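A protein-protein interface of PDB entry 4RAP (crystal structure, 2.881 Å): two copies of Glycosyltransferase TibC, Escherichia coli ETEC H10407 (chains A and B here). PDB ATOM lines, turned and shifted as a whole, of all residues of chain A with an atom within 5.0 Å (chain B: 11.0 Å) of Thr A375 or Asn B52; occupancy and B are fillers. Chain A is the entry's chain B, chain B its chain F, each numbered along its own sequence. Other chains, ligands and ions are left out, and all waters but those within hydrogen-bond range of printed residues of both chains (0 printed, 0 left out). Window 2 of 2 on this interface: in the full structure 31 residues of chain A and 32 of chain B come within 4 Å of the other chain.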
ATOM      1  N   TRP A 232       4.949   8.256  20.020  1.00  0.00           N
ATOM      2  CA  TRP A 232       6.063   7.609  19.324  1.00  0.00           C
ATOM      3  C   TRP A 232       7.017   7.077  20.371  1.00  0.00           C
ATOM      4  O   TRP A 232       7.888   7.807  20.883  1.00  0.00           O
ATOM      5  CB  TRP A 232       6.751   8.628  18.445  1.00  0.00           C
ATOM      6  CG  TRP A 232       7.895   8.082  17.650  1.00  0.00           C
ATOM      7  CD1 TRP A 232       8.173   6.751  17.369  1.00  0.00           C
ATOM      8  CD2 TRP A 232       8.892   8.852  16.903  1.00  0.00           C
ATOM      9  NE1 TRP A 232       9.287   6.651  16.573  1.00  0.00           N
ATOM     10  CE2 TRP A 232       9.753   7.876  16.244  1.00  0.00           C
ATOM     11  CE3 TRP A 232       9.165  10.209  16.754  1.00  0.00           C
ATOM     12  CZ2 TRP A 232      10.837   8.252  15.476  1.00  0.00           C
ATOM     13  CZ3 TRP A 232      10.249  10.579  15.967  1.00  0.00           C
ATOM     14  CH2 TRP A 232      11.071   9.613  15.339  1.00  0.00           C
ATOM     15  N   ASN A 234       9.662   5.306  20.600  1.00  0.00           N
ATOM     16  CA  ASN A 234      11.044   5.002  20.360  1.00  0.00           C
ATOM     17  C   ASN A 234      11.874   5.912  21.221  1.00  0.00           C
ATOM     18  O   ASN A 234      11.682   7.119  21.220  1.00  0.00           O
ATOM     19  CB  ASN A 234      11.398   5.266  18.917  1.00  0.00           C
ATOM     20  CG  ASN A 234      12.816   4.861  18.594  1.00  0.00           C
ATOM     21  OD1 ASN A 234      13.753   5.645  18.751  1.00  0.00           O
ATOM     22  ND2 ASN A 234      12.990   3.612  18.213  1.00  0.00           N
ATOM     23  N   ASN A 335       5.521   0.840  10.426  1.00  0.00           N
ATOM     24  CA  ASN A 335       6.434  -0.289  10.379  1.00  0.00           C
ATOM     25  C   ASN A 335       5.664  -1.592  10.501  1.00  0.00           C
ATOM     26  O   ASN A 335       4.929  -1.775  11.490  1.00  0.00           O
ATOM     27  CB  ASN A 335       7.424  -0.186  11.516  1.00  0.00           C
ATOM     28  CG  ASN A 335       8.645  -1.037  11.294  1.00  0.00           C
ATOM     29  OD1 ASN A 335       8.581  -2.266  11.331  1.00  0.00           O
ATOM     30  ND2 ASN A 335       9.775  -0.381  11.053  1.00  0.00           N
ATOM     31  N   ARG A 372       8.137   1.516  18.793  1.00  0.00           N
ATOM     32  CA  ARG A 372       9.557   1.338  19.100  1.00  0.00           C
ATOM     33  C   ARG A 372      10.328   0.935  17.863  1.00  0.00           C
ATOM     34  O   ARG A 372      11.495   1.291  17.709  1.00  0.00           O
ATOM     35  CB  ARG A 372       9.731   0.297  20.201  1.00  0.00           C
ATOM     36  CG  ARG A 372       9.206   0.825  21.508  1.00  0.00           C
ATOM     37  CD  ARG A 372       9.115  -0.198  22.616  1.00  0.00           C
ATOM     38  NE  ARG A 372      10.136  -1.227  22.587  1.00  0.00           N
ATOM     39  CZ  ARG A 372      10.027  -2.355  23.276  1.00  0.00           C
ATOM     40  NH1 ARG A 372       8.948  -2.564  24.017  1.00  0.00           N
ATOM     41  NH2 ARG A 372      10.974  -3.273  23.215  1.00  0.00           N
ATOM     42  N   LEU A 373       9.666   0.206  16.973  1.00  0.00           N
ATOM     43  CA  LEU A 373      10.291  -0.190  15.734  1.00  0.00           C
ATOM     44  C   LEU A 373      10.437   0.971  14.766  1.00  0.00           C
ATOM     45  O   LEU A 373      11.158   0.870  13.786  1.00  0.00           O
ATOM     46  CB  LEU A 373       9.538  -1.358  15.089  1.00  0.00           C
ATOM     47  CG  LEU A 373       9.640  -2.680  15.863  1.00  0.00           C
ATOM     48  CD1 LEU A 373       8.808  -3.769  15.208  1.00  0.00           C
ATOM     49  CD2 LEU A 373      11.098  -3.101  15.958  1.00  0.00           C
ATOM     50  N   ILE A 374       9.754   2.074  15.022  1.00  0.00           N
ATOM     51  CA  ILE A 374       9.890   3.220  14.136  1.00  0.00           C
ATOM     52  C   ILE A 374      11.055   4.070  14.607  1.00  0.00           C
ATOM     53  O   ILE A 374      10.933   4.838  15.548  1.00  0.00           O
ATOM     54  CB  ILE A 374       8.612   4.074  14.073  1.00  0.00           C
ATOM     55  CG1 ILE A 374       7.453   3.258  13.529  1.00  0.00           C
ATOM     56  CG2 ILE A 374       8.837   5.292  13.185  1.00  0.00           C
ATOM     57  CD1 ILE A 374       6.160   4.039  13.468  1.00  0.00           C
ATOM     58  N   THR A 375      12.188   3.928  13.950  1.00  0.00           N
ATOM     59  CA  THR A 375      13.388   4.615  14.376  1.00  0.00           C
ATOM     60  C   THR A 375      13.464   6.038  13.883  1.00  0.00           C
ATOM     61  O   THR A 375      12.728   6.444  12.998  1.00  0.00           O
ATOM     62  CB  THR A 375      14.618   3.898  13.858  1.00  0.00           C
ATOM     63  OG1 THR A 375      14.635   3.984  12.427  1.00  0.00           O
ATOM     64  CG2 THR A 375      14.583   2.440  14.293  1.00  0.00           C
ATOM     65  N   GLY A 376      14.379   6.794  14.461  1.00  0.00           N
ATOM     66  CA  GLY A 376      14.592   8.164  14.049  1.00  0.00           C
ATOM     67  C   GLY A 376      15.098   8.183  12.632  1.00  0.00           C
ATOM     68  O   GLY A 376      14.724   9.071  11.837  1.00  0.00           O
ATOM     69  N   ALA A 377      15.950   7.196  12.318  1.00  0.00           N
ATOM     70  CA  ALA A 377      16.479   7.011  10.967  1.00  0.00           C
ATOM     71  C   ALA A 377      15.331   6.897   9.971  1.00  0.00           C
ATOM     72  O   ALA A 377      15.316   7.572   8.929  1.00  0.00           O
ATOM     73  CB  ALA A 377      17.332   5.752  10.914  1.00  0.00           C
ATOM     74  N   GLN A 378      14.364   6.047  10.314  1.00  0.00           N
ATOM     75  CA  GLN A 378      13.211   5.844   9.474  1.00  0.00           C
ATOM     76  C   GLN A 378      12.486   7.141   9.224  1.00  0.00           C
ATOM     77  O   GLN A 378      12.155   7.456   8.079  1.00  0.00           O
ATOM     78  CB  GLN A 378      12.258   4.807  10.068  1.00  0.00           C
ATOM     79  CG  GLN A 378      11.091   4.506   9.146  1.00  0.00           C
ATOM     80  CD  GLN A 378      10.182   3.431   9.687  1.00  0.00           C
ATOM     81  OE1 GLN A 378      10.560   2.653  10.596  1.00  0.00           O
ATOM     82  NE2 GLN A 378       8.961   3.368   9.136  1.00  0.00           N
ATOM     83  N   VAL A 379      12.230   7.899  10.281  1.00  0.00           N
ATOM     84  CA  VAL A 379      11.475   9.139  10.115  1.00  0.00           C
ATOM     85  C   VAL A 379      12.302  10.188   9.376  1.00  0.00           C
ATOM     86  O   VAL A 379      11.761  10.937   8.560  1.00  0.00           O
ATOM     87  CB  VAL A 379      10.941   9.703  11.456  1.00  0.00           C
ATOM     88  CG1 VAL A 379      10.337  11.089  11.273  1.00  0.00           C
ATOM     89  CG2 VAL A 379       9.942   8.742  12.072  1.00  0.00           C
ATOM     90  N   VAL B  43      25.166 -14.322  10.550  1.00  0.00           N
ATOM     91  CA  VAL B  43      24.542 -13.456   9.518  1.00  0.00           C
ATOM     92  C   VAL B  43      23.425 -12.583  10.056  1.00  0.00           C
ATOM     93  O   VAL B  43      22.678 -12.979  10.950  1.00  0.00           O
ATOM     94  CB  VAL B  43      23.990 -14.248   8.313  1.00  0.00           C
ATOM     95  CG1 VAL B  43      25.088 -15.078   7.669  1.00  0.00           C
ATOM     96  CG2 VAL B  43      22.826 -15.122   8.744  1.00  0.00           C
ATOM     97  N   ARG B  44      23.299 -11.393   9.493  1.00  0.00           N
ATOM     98  CA  ARG B  44      22.288 -10.483   9.974  1.00  0.00           C
ATOM     99  C   ARG B  44      21.523  -9.779   8.847  1.00  0.00           C
ATOM    100  O   ARG B  44      22.106  -9.367   7.827  1.00  0.00           O
ATOM    101  CB  ARG B  44      22.863  -9.518  11.030  1.00  0.00           C
ATOM    102  CG  ARG B  44      23.292  -8.151  10.543  1.00  0.00           C
ATOM    103  CD  ARG B  44      23.258  -7.189  11.723  1.00  0.00           C
ATOM    104  NE  ARG B  44      24.426  -7.275  12.585  1.00  0.00           N
ATOM    105  CZ  ARG B  44      25.385  -6.351  12.638  1.00  0.00           C
ATOM    106  NH1 ARG B  44      25.329  -5.258  11.876  1.00  0.00           N
ATOM    107  NH2 ARG B  44      26.416  -6.525  13.451  1.00  0.00           N
ATOM    108  N   LEU B  45      20.202  -9.720   9.015  1.00  0.00           N
ATOM    109  CA  LEU B  45      19.317  -9.069   8.061  1.00  0.00           C
ATOM    110  C   LEU B  45      18.856  -7.746   8.646  1.00  0.00           C
ATOM    111  O   LEU B  45      18.386  -7.705   9.782  1.00  0.00           O
ATOM    112  CB  LEU B  45      18.095  -9.949   7.771  1.00  0.00           C
ATOM    113  CG  LEU B  45      18.247 -11.313   7.076  1.00  0.00           C
ATOM    114  CD1 LEU B  45      19.447 -11.299   6.134  1.00  0.00           C
ATOM    115  CD2 LEU B  45      18.323 -12.479   8.072  1.00  0.00           C
ATOM    116  N   LEU B  46      18.994  -6.671   7.875  1.00  0.00           N
ATOM    117  CA  LEU B  46      18.584  -5.345   8.333  1.00  0.00           C
ATOM    118  C   LEU B  46      17.612  -4.664   7.379  1.00  0.00           C
ATOM    119  O   LEU B  46      17.537  -4.997   6.200  1.00  0.00           O
ATOM    120  CB  LEU B  46      19.805  -4.451   8.489  1.00  0.00           C
ATOM    121  CG  LEU B  46      20.873  -4.974   9.427  1.00  0.00           C
ATOM    122  CD1 LEU B  46      22.199  -4.985   8.689  1.00  0.00           C
ATOM    123  CD2 LEU B  46      20.927  -4.156  10.712  1.00  0.00           C
ATOM    124  N   ASP B  47      16.864  -3.706   7.903  1.00  0.00           N
ATOM    125  CA  ASP B  47      15.998  -2.899   7.083  1.00  0.00           C
ATOM    126  C   ASP B  47      16.759  -1.592   6.897  1.00  0.00           C
ATOM    127  O   ASP B  47      16.943  -0.844   7.843  1.00  0.00           O
ATOM    128  CB  ASP B  47      14.658  -2.667   7.803  1.00  0.00           C
ATOM    129  CG  ASP B  47      13.620  -1.927   6.943  1.00  0.00           C
ATOM    130  OD1 ASP B  47      13.986  -1.185   5.991  1.00  0.00           O
ATOM    131  OD2 ASP B  47      12.415  -2.074   7.256  1.00  0.00           O
ATOM    132  N   ALA B  48      17.230  -1.339   5.686  1.00  0.00           N
ATOM    133  CA  ALA B  48      18.001  -0.138   5.413  1.00  0.00           C
ATOM    134  C   ALA B  48      17.282   1.156   5.781  1.00  0.00           C
ATOM    135  O   ALA B  48      17.916   2.121   6.188  1.00  0.00           O
ATOM    136  CB  ALA B  48      18.428  -0.101   3.957  1.00  0.00           C
ATOM    137  N   ASP B  49      15.967   1.190   5.612  1.00  0.00           N
ATOM    138  CA  ASP B  49      15.200   2.413   5.888  1.00  0.00           C
ATOM    139  C   ASP B  49      15.129   2.770   7.378  1.00  0.00           C
ATOM    140  O   ASP B  49      15.297   3.928   7.748  1.00  0.00           O
ATOM    141  CB  ASP B  49      13.807   2.338   5.258  1.00  0.00           C
ATOM    142  CG  ASP B  49      13.842   2.514   3.721  1.00  0.00           C
ATOM    143  OD1 ASP B  49      14.716   3.271   3.219  1.00  0.00           O
ATOM    144  OD2 ASP B  49      12.992   1.903   3.020  1.00  0.00           O
ATOM    145  N   SER B  50      14.956   1.754   8.224  1.00  0.00           N
ATOM    146  CA  SER B  50      14.859   1.942   9.670  1.00  0.00           C
ATOM    147  C   SER B  50      16.148   1.610  10.412  1.00  0.00           C
ATOM    148  O   SER B  50      16.328   2.023  11.560  1.00  0.00           O
ATOM    149  CB  SER B  50      13.736   1.075  10.238  1.00  0.00           C
ATOM    150  OG  SER B  50      14.023  -0.305  10.090  1.00  0.00           O
ATOM    151  N   GLU B  51      17.031   0.854   9.758  1.00  0.00           N
ATOM    152  CA  GLU B  51      18.280   0.346  10.369  1.00  0.00           C
ATOM    153  C   GLU B  51      18.028  -0.700  11.462  1.00  0.00           C
ATOM    154  O   GLU B  51      18.936  -1.051  12.219  1.00  0.00           O
ATOM    155  CB  GLU B  51      19.171   1.474  10.889  1.00  0.00           C
ATOM    156  CG  GLU B  51      19.219   2.673   9.974  1.00  0.00           C
ATOM    157  CD  GLU B  51      20.295   3.668  10.368  1.00  0.00           C
ATOM    158  OE1 GLU B  51      20.586   3.793  11.582  1.00  0.00           O
ATOM    159  OE2 GLU B  51      20.844   4.334   9.459  1.00  0.00           O
ATOM    160  N   ASN B  52      16.804  -1.210  11.525  1.00  0.00           N
ATOM    161  CA  ASN B  52      16.467  -2.268  12.485  1.00  0.00           C
ATOM    162  C   ASN B  52      17.101  -3.599  12.118  1.00  0.00           C
ATOM    163  O   ASN B  52      17.208  -3.939  10.928  1.00  0.00           O
ATOM    164  CB  ASN B  52      14.949  -2.465  12.579  1.00  0.00           C
ATOM    165  CG  ASN B  52      14.272  -1.405  13.409  1.00  0.00           C
ATOM    166  OD1 ASN B  52      14.913  -0.708  14.185  1.00  0.00           O
ATOM    167  ND2 ASN B  52      12.962  -1.297  13.270  1.00  0.00           N
ATOM    168  N   ILE B  53      17.517  -4.349  13.138  1.00  0.00           N
ATOM    169  CA  ILE B  53      18.008  -5.709  12.938  1.00  0.00           C
ATOM    170  C   ILE B  53      16.792  -6.624  12.872  1.00  0.00           C
ATOM    171  O   ILE B  53      16.198  -6.924  13.890  1.00  0.00           O
ATOM    172  CB  ILE B  53      18.903  -6.169  14.112  1.00  0.00           C
ATOM    173  CG1 ILE B  53      20.102  -5.212  14.306  1.00  0.00           C
ATOM    174  CG2 ILE B  53      19.338  -7.619  13.918  1.00  0.00           C
ATOM    175  CD1 ILE B  53      20.675  -5.191  15.722  1.00  0.00           C
ATOM    176  N   LEU B  54      16.427  -7.060  11.672  1.00  0.00           N
ATOM    177  CA  LEU B  54      15.237  -7.896  11.478  1.00  0.00           C
ATOM    178  C   LEU B  54      15.403  -9.298  12.035  1.00  0.00           C
ATOM    179  O   LEU B  54      14.477  -9.860  12.619  1.00  0.00           O
ATOM    180  CB  LEU B  54      14.916  -7.997   9.989  1.00  0.00           C
ATOM    181  CG  LEU B  54      14.008  -6.989   9.287  1.00  0.00           C
ATOM    182  CD1 LEU B  54      13.712  -5.749  10.124  1.00  0.00           C
ATOM    183  CD2 LEU B  54      14.590  -6.641   7.921  1.00  0.00           C
ATOM    184  N   PHE B  55      16.594  -9.855  11.840  1.00  0.00           N
ATOM    185  CA  PHE B  55      16.883 -11.233  12.196  1.00  0.00           C
ATOM    186  C   PHE B  55      18.399 -11.408  12.280  1.00  0.00           C
ATOM    187  O   PHE B  55      19.145 -10.800  11.501  1.00  0.00           O
ATOM    188  CB  PHE B  55      16.314 -12.139  11.101  1.00  0.00           C
ATOM    189  CG  PHE B  55      16.395 -13.599  11.407  1.00  0.00           C
ATOM    190  CD1 PHE B  55      15.588 -14.168  12.399  1.00  0.00           C
ATOM    191  CD2 PHE B  55      17.224 -14.425  10.658  1.00  0.00           C
ATOM    192  CE1 PHE B  55      15.641 -15.526  12.662  1.00  0.00           C
ATOM    193  CE2 PHE B  55      17.275 -15.784  10.909  1.00  0.00           C
ATOM    194  CZ  PHE B  55      16.486 -16.338  11.915  1.00  0.00           C
ATOM    195  N   CYS B  56      18.857 -12.222  13.229  1.00  0.00           N
ATOM    196  CA  CYS B  56      20.290 -12.511  13.347  1.00  0.00           C
ATOM    197  C   CYS B  56      20.551 -13.942  13.854  1.00  0.00           C
ATOM    198  O   CYS B  56      19.802 -14.470  14.676  1.00  0.00           O
ATOM    199  CB  CYS B  56      21.015 -11.437  14.177  1.00  0.00           C
ATOM    200  SG  CYS B  56      21.288 -11.780  15.928  1.00  0.00           S
ATOM    201  N   SER B  66      14.779 -14.494   4.910  1.00  0.00           N
ATOM    202  CA  SER B  66      13.998 -13.550   5.713  1.00  0.00           C
ATOM    203  C   SER B  66      12.600 -14.118   5.794  1.00  0.00           C
ATOM    204  O   SER B  66      12.111 -14.700   4.818  1.00  0.00           O
ATOM    205  CB  SER B  66      13.962 -12.163   5.066  1.00  0.00           C
ATOM    206  OG  SER B  66      13.227 -12.186   3.856  1.00  0.00           O
ATOM    207  N   LYS B  68      10.015 -12.295   6.102  1.00  0.00           N
ATOM    208  CA  LYS B  68       9.216 -11.368   5.289  1.00  0.00           C
ATOM    209  C   LYS B  68       9.505 -11.551   3.798  1.00  0.00           C
ATOM    210  O   LYS B  68      10.659 -11.511   3.377  1.00  0.00           O
ATOM    211  CB  LYS B  68       9.463  -9.897   5.681  1.00  0.00           C
ATOM    212  CG  LYS B  68       8.861  -9.416   7.011  1.00  0.00           C
ATOM    213  CD  LYS B  68       7.663 -10.229   7.477  1.00  0.00           C
ATOM    214  CE  LYS B  68       7.072  -9.672   8.771  1.00  0.00           C
ATOM    215  NZ  LYS B  68       7.784 -10.155   9.993  1.00  0.00           N
ATOM    216  N   TYR B  70       7.538  -9.734   1.286  1.00  0.00           N
ATOM    217  CA  TYR B  70       7.114  -8.546   0.520  1.00  0.00           C
ATOM    218  C   TYR B  70       8.285  -7.584   0.399  1.00  0.00           C
ATOM    219  O   TYR B  70       9.356  -7.853   0.934  1.00  0.00           O
ATOM    220  CB  TYR B  70       5.886  -7.861   1.151  1.00  0.00           C
ATOM    221  CG  TYR B  70       6.025  -7.603   2.638  1.00  0.00           C
ATOM    222  CD1 TYR B  70       6.684  -6.459   3.115  1.00  0.00           C
ATOM    223  CD2 TYR B  70       5.507  -8.507   3.566  1.00  0.00           C
ATOM    224  CE1 TYR B  70       6.836  -6.236   4.478  1.00  0.00           C
ATOM    225  CE2 TYR B  70       5.649  -8.289   4.929  1.00  0.00           C
ATOM    226  CZ  TYR B  70       6.316  -7.157   5.384  1.00  0.00           C
ATOM    227  OH  TYR B  70       6.437  -6.944   6.745  1.00  0.00           O
ATOM    228  N   VAL B  72      11.009  -5.010   0.974  1.00  0.00           N
ATOM    229  CA  VAL B  72      11.720  -4.383   2.095  1.00  0.00           C
ATOM    230  C   VAL B  72      13.081  -4.026   1.521  1.00  0.00           C
ATOM    231  O   VAL B  72      13.652  -4.819   0.764  1.00  0.00           O
ATOM    232  CB  VAL B  72      11.955  -5.381   3.261  1.00  0.00           C
ATOM    233  CG1 VAL B  72      12.775  -4.744   4.363  1.00  0.00           C
ATOM    234  CG2 VAL B  72      10.644  -5.939   3.793  1.00  0.00           C
ATOM    235  N   ARG B  73      13.606  -2.846   1.841  1.00  0.00           N
ATOM    236  CA  ARG B  73      14.950  -2.494   1.368  1.00  0.00           C
ATOM    237  C   ARG B  73      15.930  -3.184   2.306  1.00  0.00           C
ATOM    238  O   ARG B  73      16.526  -2.558   3.177  1.00  0.00           O
ATOM    239  CB  ARG B  73      15.175  -0.986   1.365  1.00  0.00           C
ATOM    240  CG  ARG B  73      15.901  -0.470   0.137  1.00  0.00           C
ATOM    241  CD  ARG B  73      16.046   1.039   0.182  1.00  0.00           C
ATOM    242  NE  ARG B  73      17.279   1.440   0.864  1.00  0.00           N
ATOM    243  CZ  ARG B  73      17.431   2.568   1.563  1.00  0.00           C
ATOM    244  NH1 ARG B  73      16.405   3.398   1.733  1.00  0.00           N
ATOM    245  NH2 ARG B  73      18.598   2.843   2.133  1.00  0.00           N
ATOM    246  N   PHE B  74      16.050  -4.497   2.150  1.00  0.00           N
ATOM    247  CA  PHE B  74      16.908  -5.305   2.994  1.00  0.00           C
ATOM    248  C   PHE B  74      18.386  -4.924   2.900  1.00  0.00           C
ATOM    249  O   PHE B  74      18.834  -4.357   1.907  1.00  0.00           O
ATOM    250  CB  PHE B  74      16.783  -6.755   2.591  1.00  0.00           C
ATOM    251  CG  PHE B  74      15.477  -7.388   2.951  1.00  0.00           C
ATOM    252  CD1 PHE B  74      15.239  -7.828   4.258  1.00  0.00           C
ATOM    253  CD2 PHE B  74      14.532  -7.670   1.962  1.00  0.00           C
ATOM    254  CE1 PHE B  74      14.063  -8.486   4.575  1.00  0.00           C
ATOM    255  CE2 PHE B  74      13.358  -8.340   2.272  1.00  0.00           C
ATOM    256  CZ  PHE B  74      13.122  -8.749   3.579  1.00  0.00           C
ATOM    257  N   ARG B  75      19.135  -5.286   3.938  1.00  0.00           N
ATOM    258  CA  ARG B  75      20.586  -5.122   3.978  1.00  0.00           C
ATOM    259  C   ARG B  75      21.193  -6.402   4.573  1.00  0.00           C
ATOM    260  O   ARG B  75      20.946  -6.736   5.742  1.00  0.00           O
ATOM    261  CB  ARG B  75      20.946  -3.909   4.826  1.00  0.00           C
ATOM    262  CG  ARG B  75      22.418  -3.579   4.870  1.00  0.00           C
ATOM    263  CD  ARG B  75      22.683  -2.389   5.780  1.00  0.00           C
ATOM    264  NE  ARG B  75      24.100  -2.023   5.800  1.00  0.00           N
ATOM    265  CZ  ARG B  75      24.617  -1.027   6.518  1.00  0.00           C
ATOM    266  NH1 ARG B  75      23.844  -0.274   7.290  1.00  0.00           N
ATOM    267  NH2 ARG B  75      25.916  -0.786   6.462  1.00  0.00           N
ATOM    268  N   ILE B  76      21.999  -7.105   3.789  1.00  0.00           N
ATOM    269  CA  ILE B  76      22.538  -8.377   4.243  1.00  0.00           C
ATOM    270  C   ILE B  76      23.951  -8.256   4.785  1.00  0.00           C
ATOM    271  O   ILE B  76      24.831  -7.692   4.141  1.00  0.00           O
ATOM    272  CB  ILE B  76      22.539  -9.423   3.126  1.00  0.00           C
ATOM    273  CG1 ILE B  76      21.308  -9.256   2.240  1.00  0.00           C
ATOM    274  CG2 ILE B  76      22.569 -10.815   3.717  1.00  0.00           C
ATOM    275  CD1 ILE B  76      20.760 -10.561   1.726  1.00  0.00           C
ATOM    276  N   GLN B  77      24.153  -8.782   5.985  1.00  0.00           N
ATOM    277  CA  GLN B  77      25.472  -8.817   6.588  1.00  0.00           C
ATOM    278  C   GLN B  77      25.861 -10.241   6.949  1.00  0.00           C
ATOM    279  O   GLN B  77      25.107 -10.952   7.610  1.00  0.00           O
ATOM    280  CB  GLN B  77      25.511  -7.934   7.832  1.00  0.00           C
ATOM    281  CG  GLN B  77      24.981  -6.539   7.597  1.00  0.00           C
ATOM    282  CD  GLN B  77      25.628  -5.515   8.491  1.00  0.00           C
ATOM    283  OE1 GLN B  77      25.602  -5.641   9.712  1.00  0.00           O
ATOM    284  NE2 GLN B  77      26.212  -4.491   7.888  1.00  0.00           N
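Printed residues of chain A that touch a printed residue of chain B: Asn A335, Leu A373, Thr A375, Ala A377 and Gln A378. Among the printed residues, no Asp or Glu carboxylate lies within 4 Å of a Lys or Arg side-chain nitrogen of the other chain.
ND2 of Asn A335 lies within hydrogen-bond range of O of Leu A373 (3.3 Å). N of Ala A377 sits close to OG1 of Thr A375 (3.5 Å). The side-chain hydroxyl (OG1) of Thr A375 sits at hydrogen-bond distance from the backbone NH (N) of Gln A378, at 3.0 Å. N of Asp B49 is in hydrogen-bond range of OD1 of Asp B47 (3.1 Å). N of Asp B47 is in hydrogen-bond range of O of Asn B52. OD1 of Asp B49 is in salt-bridge range of NE of Arg B73, 3.9 Å away.
No position is printed for both chains. Of the 9 pairs that touch across the chains among the printed residues, none has its exchanged pair printed and touching as well.
Among the printed residues, merely in contact across the chains: Asn A335 with Asn B52, Thr A375 with Asn B52, Ala A377 with Asp B49, Ala A377 with Ser B50, Ala A377 with Glu B51 and Gln A378 with Ser B50.
Of the printed residues of chain B, Asn A335 touches Asn B52 (3.99 Å). No residue of chain B comes within 4 Å of Ile A374. Thr A375 touches just these residues of chain B: Ser B50 and Asn B52. No residue of chain B comes within 4 Å of Gly A376. Of chain B, only Asp B49, Ser B50 and Glu B51 come within 4 Å of Ala A377. Of chain B, only Asp B49 (3.3 Å) and Ser B50 (3.6 Å) come within 4 Å of Gln A378. Val A379 touches none of the printed residues of chain B. Of the printed residues of chain A, Asp B49 touches Ala A377 and Gln A378. Printed residues of chain A within 4 Å of Ser B50: Thr A375 (2.7 Å), Ala A377 (3.9 Å) and Gln A378 (3.6 Å). Of the printed residues of chain A, Glu B51 touches Ala A377 (3.7 Å). Printed residues of chain A within 4 Å of Asn B52: Asn A335 (3.99 Å), Leu A373 (2.9 Å) and Thr A375 (3.2 Å). Arg B73 touches none of the printed residues of chain A. The nearest printed residue of chain A that does not touch Asn B52 is Ile A374 (5.0 Å).
The side-chain amide nitrogen of Asn B52 sits at hydrogen-bond distance from the backbone carbonyl oxygen of Leu A373 (2.9 Å). The backbone carbonyl oxygen of Ser B50 is in hydrogen-bond range of the side-chain hydroxyl of Thr A375 (2.7 Å). The backbone carbonyl oxygen (O) of Asp B49 sits close to the backbone NH (N) of Gln A378 (3.5 Å).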
